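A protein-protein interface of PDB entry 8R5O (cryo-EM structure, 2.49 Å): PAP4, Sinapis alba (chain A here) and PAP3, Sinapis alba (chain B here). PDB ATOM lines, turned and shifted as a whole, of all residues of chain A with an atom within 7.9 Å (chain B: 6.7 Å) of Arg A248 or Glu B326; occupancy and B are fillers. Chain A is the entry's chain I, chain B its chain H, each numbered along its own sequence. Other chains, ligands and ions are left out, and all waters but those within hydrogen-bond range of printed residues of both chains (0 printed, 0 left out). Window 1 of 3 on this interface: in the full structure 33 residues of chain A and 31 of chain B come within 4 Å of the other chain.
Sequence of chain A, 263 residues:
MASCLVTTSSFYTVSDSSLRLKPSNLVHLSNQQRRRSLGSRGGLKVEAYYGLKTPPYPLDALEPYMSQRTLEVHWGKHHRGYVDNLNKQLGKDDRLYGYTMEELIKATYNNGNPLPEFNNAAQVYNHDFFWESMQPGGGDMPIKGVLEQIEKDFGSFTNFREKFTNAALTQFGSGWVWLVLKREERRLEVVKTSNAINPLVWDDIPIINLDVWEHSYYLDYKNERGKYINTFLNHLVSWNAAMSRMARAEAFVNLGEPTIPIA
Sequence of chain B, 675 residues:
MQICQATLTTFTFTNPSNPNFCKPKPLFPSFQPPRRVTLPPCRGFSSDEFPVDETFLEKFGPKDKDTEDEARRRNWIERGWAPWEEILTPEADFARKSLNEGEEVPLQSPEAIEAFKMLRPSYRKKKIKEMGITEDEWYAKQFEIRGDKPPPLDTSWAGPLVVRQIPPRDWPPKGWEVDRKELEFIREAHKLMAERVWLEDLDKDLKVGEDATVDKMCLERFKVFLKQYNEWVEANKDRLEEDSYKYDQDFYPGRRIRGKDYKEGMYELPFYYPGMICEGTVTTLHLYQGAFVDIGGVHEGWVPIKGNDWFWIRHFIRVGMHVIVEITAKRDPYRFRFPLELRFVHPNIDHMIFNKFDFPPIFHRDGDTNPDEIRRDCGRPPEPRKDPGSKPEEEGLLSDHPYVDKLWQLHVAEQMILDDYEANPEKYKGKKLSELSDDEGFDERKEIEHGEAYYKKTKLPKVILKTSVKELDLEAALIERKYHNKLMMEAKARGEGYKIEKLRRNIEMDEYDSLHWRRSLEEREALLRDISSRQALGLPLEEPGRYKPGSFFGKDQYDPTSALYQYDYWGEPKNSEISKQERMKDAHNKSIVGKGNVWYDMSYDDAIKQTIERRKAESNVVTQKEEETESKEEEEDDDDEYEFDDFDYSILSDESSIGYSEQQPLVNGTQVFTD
OE1 of Glu B326 is in salt-bridge range of NH1 of Arg B343 (3.4 Å).
The guanidinium group (NH2) of Arg B343 lies within salt-bridge range of the side-chain carboxylate (OD2) of Asp B350, at 2.7 Å.
Printed residues of chain A that touch a printed residue of chain B: Arg A248, Glu A250 and Ala A251.
Hydrophobic or aromatic side chains of chain A within 4 Å of the printed part of chain B: Ala A251.
Along chain A the printed residues that touch a printed residue of chain B span positions 248 to 251.
Among the printed residues, 5 pairs touch across the chains.
Among the printed residues, Asp or Glu carboxylates within 4 Å of a Lys or Arg side-chain nitrogen of the other chain: Arg A248 with Glu B326 (3.5 Å).
Among the printed residues, pairs that only touch across the chains: Arg A248 with Arg B343, Glu A250 with Asp B350, Ala A251 with Arg B343 and Ala A251 with Asp B350.
Of chain B, only Glu B326 and Arg B343 come within 4 Å of Arg A248.
Glu B326 touches one residue of chain A.
Printed residues of chain B within 4 Å of Glu A250: Asp B350 (3.9 Å).
Printed residues of chain A within 4 Å of Asp B350: Glu A250 (3.9 Å) and Ala A251 (3.4 Å).
The nearest residue of chain B that does not touch Arg A248 is Thr B328 (5.5 Å).
The side-chain carboxylate of Glu B326 is in salt-bridge range of the guanidinium group of Arg A248 (3.5 Å).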
ATOM      1  N   GLU A 102     -15.089  -1.371 -16.544  1.00  0.00           N
ATOM      2  CA  GLU A 102     -14.152  -0.614 -17.368  1.00  0.00           C
ATOM      3  C   GLU A 102     -13.970   0.802 -16.835  1.00  0.00           C
ATOM      4  O   GLU A 102     -12.844   1.308 -16.773  1.00  0.00           O
ATOM      5  CB  GLU A 102     -14.636  -0.581 -18.819  1.00  0.00           C
ATOM      6  CG  GLU A 102     -15.331  -1.854 -19.284  1.00  0.00           C
ATOM      7  CD  GLU A 102     -16.803  -1.889 -18.910  1.00  0.00           C
ATOM      8  OE1 GLU A 102     -17.411  -0.806 -18.785  1.00  0.00           O
ATOM      9  OE2 GLU A 102     -17.346  -2.997 -18.730  1.00  0.00           O
ATOM     10  N   LEU A 181      -6.133  -3.835 -29.696  1.00  0.00           N
ATOM     11  CA  LEU A 181      -6.611  -3.081 -30.844  1.00  0.00           C
ATOM     12  C   LEU A 181      -6.530  -1.601 -30.500  1.00  0.00           C
ATOM     13  O   LEU A 181      -7.210  -1.137 -29.579  1.00  0.00           O
ATOM     14  CB  LEU A 181      -8.040  -3.476 -31.208  1.00  0.00           C
ATOM     15  CG  LEU A 181      -8.580  -2.901 -32.516  1.00  0.00           C
ATOM     16  CD1 LEU A 181      -7.729  -3.365 -33.687  1.00  0.00           C
ATOM     17  CD2 LEU A 181     -10.030  -3.293 -32.717  1.00  0.00           C
ATOM     18  N   ILE A 205      -8.423  -1.611 -26.619  1.00  0.00           N
ATOM     19  CA  ILE A 205      -9.323  -2.750 -26.483  1.00  0.00           C
ATOM     20  C   ILE A 205      -8.477  -4.022 -26.473  1.00  0.00           C
ATOM     21  O   ILE A 205      -7.893  -4.384 -27.506  1.00  0.00           O
ATOM     22  CB  ILE A 205     -10.374  -2.789 -27.600  1.00  0.00           C
ATOM     23  CG1 ILE A 205     -11.290  -1.564 -27.532  1.00  0.00           C
ATOM     24  CG2 ILE A 205     -11.202  -4.057 -27.501  1.00  0.00           C
ATOM     25  CD1 ILE A 205     -10.822  -0.394 -28.362  1.00  0.00           C
ATOM     26  N   ILE A 207      -7.480  -7.923 -26.761  1.00  0.00           N
ATOM     27  CA  ILE A 207      -7.948  -9.021 -27.597  1.00  0.00           C
ATOM     28  C   ILE A 207      -7.515 -10.372 -27.039  1.00  0.00           C
ATOM     29  O   ILE A 207      -8.331 -11.287 -26.896  1.00  0.00           O
ATOM     30  CB  ILE A 207      -7.474  -8.857 -29.060  1.00  0.00           C
ATOM     31  CG1 ILE A 207      -7.868  -7.479 -29.600  1.00  0.00           C
ATOM     32  CG2 ILE A 207      -8.054  -9.953 -29.935  1.00  0.00           C
ATOM     33  CD1 ILE A 207      -9.361  -7.230 -29.629  1.00  0.00           C
ATOM     34  N   ALA A 241     -12.069 -16.962 -29.013  1.00  0.00           N
ATOM     35  CA  ALA A 241     -12.367 -15.813 -28.162  1.00  0.00           C
ATOM     36  C   ALA A 241     -11.936 -14.515 -28.828  1.00  0.00           C
ATOM     37  O   ALA A 241     -12.631 -13.497 -28.731  1.00  0.00           O
ATOM     38  CB  ALA A 241     -11.685 -15.972 -26.804  1.00  0.00           C
ATOM     39  N   ALA A 242     -10.789 -14.533 -29.512  1.00  0.00           N
ATOM     40  CA  ALA A 242     -10.321 -13.343 -30.211  1.00  0.00           C
ATOM     41  C   ALA A 242     -11.280 -12.923 -31.316  1.00  0.00           C
ATOM     42  O   ALA A 242     -11.445 -11.726 -31.567  1.00  0.00           O
ATOM     43  CB  ALA A 242      -8.924 -13.585 -30.780  1.00  0.00           C
ATOM     44  N   MET A 243     -11.921 -13.887 -31.982  1.00  0.00           N
ATOM     45  CA  MET A 243     -12.890 -13.557 -33.023  1.00  0.00           C
ATOM     46  C   MET A 243     -14.038 -12.728 -32.464  1.00  0.00           C
ATOM     47  O   MET A 243     -14.439 -11.719 -33.052  1.00  0.00           O
ATOM     48  CB  MET A 243     -13.421 -14.838 -33.668  1.00  0.00           C
ATOM     49  CG  MET A 243     -12.370 -15.653 -34.400  1.00  0.00           C
ATOM     50  SD  MET A 243     -12.339 -15.337 -36.172  1.00  0.00           S
ATOM     51  CE  MET A 243     -13.823 -16.193 -36.685  1.00  0.00           C
ATOM     52  N   SER A 244     -14.578 -13.139 -31.315  1.00  0.00           N
ATOM     53  CA  SER A 244     -15.710 -12.428 -30.735  1.00  0.00           C
ATOM     54  C   SER A 244     -15.293 -11.095 -30.127  1.00  0.00           C
ATOM     55  O   SER A 244     -16.065 -10.132 -30.168  1.00  0.00           O
ATOM     56  CB  SER A 244     -16.387 -13.297 -29.682  1.00  0.00           C
ATOM     57  OG  SER A 244     -16.914 -14.480 -30.254  1.00  0.00           O
ATOM     58  N   ARG A 245     -14.094 -11.025 -29.551  1.00  0.00           N
ATOM     59  CA  ARG A 245     -13.626  -9.770 -28.979  1.00  0.00           C
ATOM     60  C   ARG A 245     -13.364  -8.732 -30.061  1.00  0.00           C
ATOM     61  O   ARG A 245     -13.605  -7.538 -29.852  1.00  0.00           O
ATOM     62  CB  ARG A 245     -12.370 -10.012 -28.146  1.00  0.00           C
ATOM     63  CG  ARG A 245     -12.645 -10.728 -26.841  1.00  0.00           C
ATOM     64  CD  ARG A 245     -11.412 -11.448 -26.357  1.00  0.00           C
ATOM     65  NE  ARG A 245     -11.565 -11.956 -25.000  1.00  0.00           N
ATOM     66  CZ  ARG A 245     -10.634 -12.641 -24.352  1.00  0.00           C
ATOM     67  NH1 ARG A 245      -9.480 -12.946 -24.919  1.00  0.00           N
ATOM     68  NH2 ARG A 245     -10.865 -13.022 -23.101  1.00  0.00           N
ATOM     69  N   MET A 246     -12.870  -9.163 -31.223  1.00  0.00           N
ATOM     70  CA  MET A 246     -12.729  -8.238 -32.341  1.00  0.00           C
ATOM     71  C   MET A 246     -14.091  -7.818 -32.876  1.00  0.00           C
ATOM     72  O   MET A 246     -14.272  -6.670 -33.296  1.00  0.00           O
ATOM     73  CB  MET A 246     -11.879  -8.861 -33.448  1.00  0.00           C
ATOM     74  CG  MET A 246     -10.428  -9.069 -33.054  1.00  0.00           C
ATOM     75  SD  MET A 246      -9.339  -9.361 -34.458  1.00  0.00           S
ATOM     76  CE  MET A 246      -9.383  -7.760 -35.256  1.00  0.00           C
ATOM     77  N   ALA A 247     -15.062  -8.735 -32.871  1.00  0.00           N
ATOM     78  CA  ALA A 247     -16.418  -8.380 -33.276  1.00  0.00           C
ATOM     79  C   ALA A 247     -17.016  -7.339 -32.340  1.00  0.00           C
ATOM     80  O   ALA A 247     -17.667  -6.390 -32.789  1.00  0.00           O
ATOM     81  CB  ALA A 247     -17.298  -9.628 -33.323  1.00  0.00           C
ATOM     82  N   ARG A 248     -16.811  -7.504 -31.032  1.00  0.00           N
ATOM     83  CA  ARG A 248     -17.259  -6.495 -30.077  1.00  0.00           C
ATOM     84  C   ARG A 248     -16.489  -5.192 -30.252  1.00  0.00           C
ATOM     85  O   ARG A 248     -17.063  -4.104 -30.137  1.00  0.00           O
ATOM     86  CB  ARG A 248     -17.113  -7.025 -28.652  1.00  0.00           C
ATOM     87  CG  ARG A 248     -17.514  -6.042 -27.567  1.00  0.00           C
ATOM     88  CD  ARG A 248     -18.977  -5.658 -27.674  1.00  0.00           C
ATOM     89  NE  ARG A 248     -19.367  -4.712 -26.634  1.00  0.00           N
ATOM     90  CZ  ARG A 248     -20.561  -4.145 -26.545  1.00  0.00           C
ATOM     91  NH1 ARG A 248     -21.515  -4.402 -27.424  1.00  0.00           N
ATOM     92  NH2 ARG A 248     -20.805  -3.298 -25.551  1.00  0.00           N
ATOM     93  N   ALA A 249     -15.187  -5.284 -30.536  1.00  0.00           N
ATOM     94  CA  ALA A 249     -14.379  -4.084 -30.724  1.00  0.00           C
ATOM     95  C   ALA A 249     -14.752  -3.341 -32.001  1.00  0.00           C
ATOM     96  O   ALA A 249     -14.580  -2.120 -32.074  1.00  0.00           O
ATOM     97  CB  ALA A 249     -12.897  -4.448 -30.741  1.00  0.00           C
ATOM     98  N   GLU A 250     -15.260  -4.050 -33.011  1.00  0.00           N
ATOM     99  CA  GLU A 250     -15.655  -3.416 -34.263  1.00  0.00           C
ATOM    100  C   GLU A 250     -16.836  -2.471 -34.099  1.00  0.00           C
ATOM    101  O   GLU A 250     -17.106  -1.681 -35.010  1.00  0.00           O
ATOM    102  CB  GLU A 250     -15.991  -4.479 -35.309  1.00  0.00           C
ATOM    103  CG  GLU A 250     -14.794  -4.984 -36.097  1.00  0.00           C
ATOM    104  CD  GLU A 250     -14.484  -4.122 -37.304  1.00  0.00           C
ATOM    105  OE1 GLU A 250     -15.118  -3.056 -37.456  1.00  0.00           O
ATOM    106  OE2 GLU A 250     -13.613  -4.514 -38.107  1.00  0.00           O
ATOM    107  N   ALA A 251     -17.540  -2.527 -32.970  1.00  0.00           N
ATOM    108  CA  ALA A 251     -18.582  -1.557 -32.672  1.00  0.00           C
ATOM    109  C   ALA A 251     -18.021  -0.199 -32.277  1.00  0.00           C
ATOM    110  O   ALA A 251     -18.802   0.743 -32.099  1.00  0.00           O
ATOM    111  CB  ALA A 251     -19.491  -2.086 -31.563  1.00  0.00           C
ATOM    112  N   PHE A 252     -16.702  -0.072 -32.131  1.00  0.00           N
ATOM    113  CA  PHE A 252     -16.091   1.181 -31.717  1.00  0.00           C
ATOM    114  C   PHE A 252     -14.902   1.616 -32.564  1.00  0.00           C
ATOM    115  O   PHE A 252     -14.469   2.764 -32.422  1.00  0.00           O
ATOM    116  CB  PHE A 252     -15.636   1.097 -30.251  1.00  0.00           C
ATOM    117  CG  PHE A 252     -16.647   0.467 -29.331  1.00  0.00           C
ATOM    118  CD1 PHE A 252     -17.725   1.195 -28.861  1.00  0.00           C
ATOM    119  CD2 PHE A 252     -16.512  -0.854 -28.934  1.00  0.00           C
ATOM    120  CE1 PHE A 252     -18.655   0.616 -28.015  1.00  0.00           C
ATOM    121  CE2 PHE A 252     -17.437  -1.437 -28.090  1.00  0.00           C
ATOM    122  CZ  PHE A 252     -18.510  -0.701 -27.628  1.00  0.00           C
ATOM    123  N   VAL A 253     -14.358   0.756 -33.429  1.00  0.00           N
ATOM    124  CA  VAL A 253     -13.118   1.039 -34.138  1.00  0.00           C
ATOM    125  C   VAL A 253     -13.308   1.071 -35.650  1.00  0.00           C
ATOM    126  O   VAL A 253     -12.744   1.938 -36.328  1.00  0.00           O
ATOM    127  CB  VAL A 253     -12.012   0.035 -33.749  1.00  0.00           C
ATOM    128  CG1 VAL A 253     -10.725   0.354 -34.483  1.00  0.00           C
ATOM    129  CG2 VAL A 253     -11.785   0.061 -32.247  1.00  0.00           C
ATOM    130  N   PRO B 274     -25.717   1.601 -17.878  1.00  0.00           N
ATOM    131  CA  PRO B 274     -25.101   0.962 -19.047  1.00  0.00           C
ATOM    132  C   PRO B 274     -25.269  -0.550 -19.021  1.00  0.00           C
ATOM    133  O   PRO B 274     -25.195  -1.188 -17.970  1.00  0.00           O
ATOM    134  CB  PRO B 274     -23.629   1.367 -18.934  1.00  0.00           C
ATOM    135  CG  PRO B 274     -23.663   2.664 -18.213  1.00  0.00           C
ATOM    136  CD  PRO B 274     -24.809   2.573 -17.243  1.00  0.00           C
ATOM    137  N   GLY B 275     -25.500  -1.119 -20.202  1.00  0.00           N
ATOM    138  CA  GLY B 275     -25.780  -2.525 -20.354  1.00  0.00           C
ATOM    139  C   GLY B 275     -27.247  -2.856 -20.541  1.00  0.00           C
ATOM    140  O   GLY B 275     -27.563  -3.956 -21.005  1.00  0.00           O
ATOM    141  N   MET B 276     -28.144  -1.939 -20.192  1.00  0.00           N
ATOM    142  CA  MET B 276     -29.568  -2.167 -20.394  1.00  0.00           C
ATOM    143  C   MET B 276     -29.912  -2.149 -21.878  1.00  0.00           C
ATOM    144  O   MET B 276     -29.325  -1.399 -22.661  1.00  0.00           O
ATOM    145  CB  MET B 276     -30.393  -1.112 -19.660  1.00  0.00           C
ATOM    146  CG  MET B 276     -30.382  -1.244 -18.151  1.00  0.00           C
ATOM    147  SD  MET B 276     -31.432  -0.018 -17.351  1.00  0.00           S
ATOM    148  CE  MET B 276     -31.160  -0.417 -15.629  1.00  0.00           C
ATOM    149  N   ILE B 277     -30.873  -2.984 -22.258  1.00  0.00           N
ATOM    150  CA  ILE B 277     -31.399  -3.030 -23.615  1.00  0.00           C
ATOM    151  C   ILE B 277     -32.757  -2.348 -23.616  1.00  0.00           C
ATOM    152  O   ILE B 277     -33.603  -2.634 -22.760  1.00  0.00           O
ATOM    153  CB  ILE B 277     -31.507  -4.478 -24.124  1.00  0.00           C
ATOM    154  CG1 ILE B 277     -30.171  -5.201 -23.957  1.00  0.00           C
ATOM    155  CG2 ILE B 277     -31.949  -4.503 -25.575  1.00  0.00           C
ATOM    156  CD1 ILE B 277     -29.027  -4.543 -24.684  1.00  0.00           C
ATOM    157  N   CYS B 278     -32.968  -1.441 -24.565  1.00  0.00           N
ATOM    158  CA  CYS B 278     -34.197  -0.669 -24.634  1.00  0.00           C
ATOM    159  C   CYS B 278     -34.785  -0.747 -26.034  1.00  0.00           C
ATOM    160  O   CYS B 278     -34.062  -0.892 -27.022  1.00  0.00           O
ATOM    161  CB  CYS B 278     -33.963   0.804 -24.264  1.00  0.00           C
ATOM    162  SG  CYS B 278     -33.082   1.073 -22.715  1.00  0.00           S
ATOM    163  N   ILE B 324     -33.904  -1.104 -31.552  1.00  0.00           N
ATOM    164  CA  ILE B 324     -33.419  -1.689 -30.310  1.00  0.00           C
ATOM    165  C   ILE B 324     -32.037  -1.114 -30.045  1.00  0.00           C
ATOM    166  O   ILE B 324     -31.154  -1.190 -30.907  1.00  0.00           O
ATOM    167  CB  ILE B 324     -33.378  -3.226 -30.378  1.00  0.00           C
ATOM    168  CG1 ILE B 324     -34.796  -3.782 -30.505  1.00  0.00           C
ATOM    169  CG2 ILE B 324     -32.683  -3.800 -29.154  1.00  0.00           C
ATOM    170  CD1 ILE B 324     -34.849  -5.277 -30.643  1.00  0.00           C
ATOM    171  N   VAL B 325     -31.852  -0.527 -28.866  1.00  0.00           N
ATOM    172  CA  VAL B 325     -30.618   0.164 -28.530  1.00  0.00           C
ATOM    173  C   VAL B 325     -30.064  -0.396 -27.227  1.00  0.00           C
ATOM    174  O   VAL B 325     -30.773  -1.011 -26.430  1.00  0.00           O
ATOM    175  CB  VAL B 325     -30.819   1.691 -28.419  1.00  0.00           C
ATOM    176  CG1 VAL B 325     -31.249   2.272 -29.756  1.00  0.00           C
ATOM    177  CG2 VAL B 325     -31.833   2.020 -27.336  1.00  0.00           C
ATOM    178  N   GLU B 326     -28.770  -0.172 -27.026  1.00  0.00           N
ATOM    179  CA  GLU B 326     -28.078  -0.532 -25.798  1.00  0.00           C
ATOM    180  C   GLU B 326     -27.442   0.713 -25.199  1.00  0.00           C
ATOM    181  O   GLU B 326     -26.827   1.511 -25.912  1.00  0.00           O
ATOM    182  CB  GLU B 326     -27.001  -1.593 -26.053  1.00  0.00           C
ATOM    183  CG  GLU B 326     -26.190  -1.952 -24.818  1.00  0.00           C
ATOM    184  CD  GLU B 326     -24.741  -2.257 -25.140  1.00  0.00           C
ATOM    185  OE1 GLU B 326     -24.436  -2.522 -26.322  1.00  0.00           O
ATOM    186  OE2 GLU B 326     -23.904  -2.221 -24.212  1.00  0.00           O
ATOM    187  N   ILE B 327     -27.591   0.877 -23.889  1.00  0.00           N
ATOM    188  CA  ILE B 327     -26.996   2.011 -23.192  1.00  0.00           C
ATOM    189  C   ILE B 327     -25.510   1.739 -23.000  1.00  0.00           C
ATOM    190  O   ILE B 327     -25.126   0.729 -22.402  1.00  0.00           O
ATOM    191  CB  ILE B 327     -27.690   2.259 -21.846  1.00  0.00           C
ATOM    192  CG1 ILE B 327     -29.180   2.521 -22.059  1.00  0.00           C
ATOM    193  CG2 ILE B 327     -27.038   3.425 -21.119  1.00  0.00           C
ATOM    194  CD1 ILE B 327     -29.963   2.632 -20.781  1.00  0.00           C
ATOM    195  N   THR B 328     -24.671   2.639 -23.511  1.00  0.00           N
ATOM    196  CA  THR B 328     -23.228   2.502 -23.370  1.00  0.00           C
ATOM    197  C   THR B 328     -22.636   3.419 -22.310  1.00  0.00           C
ATOM    198  O   THR B 328     -21.572   3.104 -21.768  1.00  0.00           O
ATOM    199  CB  THR B 328     -22.527   2.769 -24.710  1.00  0.00           C
ATOM    200  OG1 THR B 328     -22.883   4.069 -25.193  1.00  0.00           O
ATOM    201  CG2 THR B 328     -22.925   1.725 -25.739  1.00  0.00           C
ATOM    202  N   ALA B 329     -23.294   4.531 -21.996  1.00  0.00           N
ATOM    203  CA  ALA B 329     -22.799   5.437 -20.971  1.00  0.00           C
ATOM    204  C   ALA B 329     -23.954   6.274 -20.443  1.00  0.00           C
ATOM    205  O   ALA B 329     -24.883   6.609 -21.181  1.00  0.00           O
ATOM    206  CB  ALA B 329     -21.688   6.344 -21.511  1.00  0.00           C
ATOM    207  N   GLU B 341     -26.009   7.872 -23.633  1.00  0.00           N
ATOM    208  CA  GLU B 341     -25.320   7.530 -24.868  1.00  0.00           C
ATOM    209  C   GLU B 341     -25.687   6.108 -25.267  1.00  0.00           C
ATOM    210  O   GLU B 341     -25.618   5.190 -24.445  1.00  0.00           O
ATOM    211  CB  GLU B 341     -23.808   7.675 -24.706  1.00  0.00           C
ATOM    212  CG  GLU B 341     -23.038   7.583 -26.008  1.00  0.00           C
ATOM    213  CD  GLU B 341     -21.595   8.019 -25.860  1.00  0.00           C
ATOM    214  OE1 GLU B 341     -21.255   8.612 -24.815  1.00  0.00           O
ATOM    215  OE2 GLU B 341     -20.802   7.771 -26.792  1.00  0.00           O
ATOM    216  N   LEU B 342     -26.079   5.930 -26.525  1.00  0.00           N
ATOM    217  CA  LEU B 342     -26.605   4.663 -27.006  1.00  0.00           C
ATOM    218  C   LEU B 342     -25.818   4.190 -28.217  1.00  0.00           C
ATOM    219  O   LEU B 342     -25.026   4.929 -28.809  1.00  0.00           O
ATOM    220  CB  LEU B 342     -28.088   4.777 -27.385  1.00  0.00           C
ATOM    221  CG  LEU B 342     -29.072   5.403 -26.400  1.00  0.00           C
ATOM    222  CD1 LEU B 342     -30.440   5.498 -27.048  1.00  0.00           C
ATOM    223  CD2 LEU B 342     -29.139   4.593 -25.121  1.00  0.00           C
ATOM    224  N   ARG B 343     -26.050   2.931 -28.576  1.00  0.00           N
ATOM    225  CA  ARG B 343     -25.659   2.394 -29.867  1.00  0.00           C
ATOM    226  C   ARG B 343     -26.808   1.549 -30.394  1.00  0.00           C
ATOM    227  O   ARG B 343     -27.548   0.936 -29.622  1.00  0.00           O
ATOM    228  CB  ARG B 343     -24.373   1.561 -29.784  1.00  0.00           C
ATOM    229  CG  ARG B 343     -24.443   0.389 -28.826  1.00  0.00           C
ATOM    230  CD  ARG B 343     -23.193  -0.468 -28.925  1.00  0.00           C
ATOM    231  NE  ARG B 343     -23.069  -1.095 -30.236  1.00  0.00           N
ATOM    232  CZ  ARG B 343     -23.546  -2.294 -30.539  1.00  0.00           C
ATOM    233  NH1 ARG B 343     -24.178  -3.033 -29.643  1.00  0.00           N
ATOM    234  NH2 ARG B 343     -23.386  -2.762 -31.773  1.00  0.00           N
ATOM    235  N   PHE B 344     -26.961   1.529 -31.713  1.00  0.00           N
ATOM    236  CA  PHE B 344     -28.028   0.743 -32.316  1.00  0.00           C
ATOM    237  C   PHE B 344     -27.688  -0.739 -32.259  1.00  0.00           C
ATOM    238  O   PHE B 344     -26.622  -1.162 -32.717  1.00  0.00           O
ATOM    239  CB  PHE B 344     -28.267   1.174 -33.763  1.00  0.00           C
ATOM    240  CG  PHE B 344     -28.977   2.490 -33.897  1.00  0.00           C
ATOM    241  CD1 PHE B 344     -30.270   2.644 -33.430  1.00  0.00           C
ATOM    242  CD2 PHE B 344     -28.359   3.567 -34.507  1.00  0.00           C
ATOM    243  CE1 PHE B 344     -30.927   3.849 -33.555  1.00  0.00           C
ATOM    244  CE2 PHE B 344     -29.013   4.775 -34.638  1.00  0.00           C
ATOM    245  CZ  PHE B 344     -30.298   4.917 -34.160  1.00  0.00           C
ATOM    246  N   VAL B 345     -28.591  -1.527 -31.687  1.00  0.00           N
ATOM    247  CA  VAL B 345     -28.471  -2.981 -31.726  1.00  0.00           C
ATOM    248  C   VAL B 345     -29.171  -3.551 -32.948  1.00  0.00           C
ATOM    249  O   VAL B 345     -28.596  -4.346 -33.695  1.00  0.00           O
ATOM    250  CB  VAL B 345     -29.022  -3.593 -30.420  1.00  0.00           C
ATOM    251  CG1 VAL B 345     -28.973  -5.109 -30.482  1.00  0.00           C
ATOM    252  CG2 VAL B 345     -28.241  -3.076 -29.228  1.00  0.00           C
ATOM    253  N   ASP B 350     -22.695  -0.701 -37.258  1.00  0.00           N
ATOM    254  CA  ASP B 350     -21.324  -0.501 -36.798  1.00  0.00           C
ATOM    255  C   ASP B 350     -20.358  -0.374 -37.970  1.00  0.00           C
ATOM    256  O   ASP B 350     -19.402   0.407 -37.915  1.00  0.00           O
ATOM    257  CB  ASP B 350     -20.901  -1.650 -35.883  1.00  0.00           C
ATOM    258  CG  ASP B 350     -21.707  -1.705 -34.601  1.00  0.00           C
ATOM    259  OD1 ASP B 350     -22.251  -0.657 -34.192  1.00  0.00           O
ATOM    260  OD2 ASP B 350     -21.792  -2.794 -33.998  1.00  0.00           O
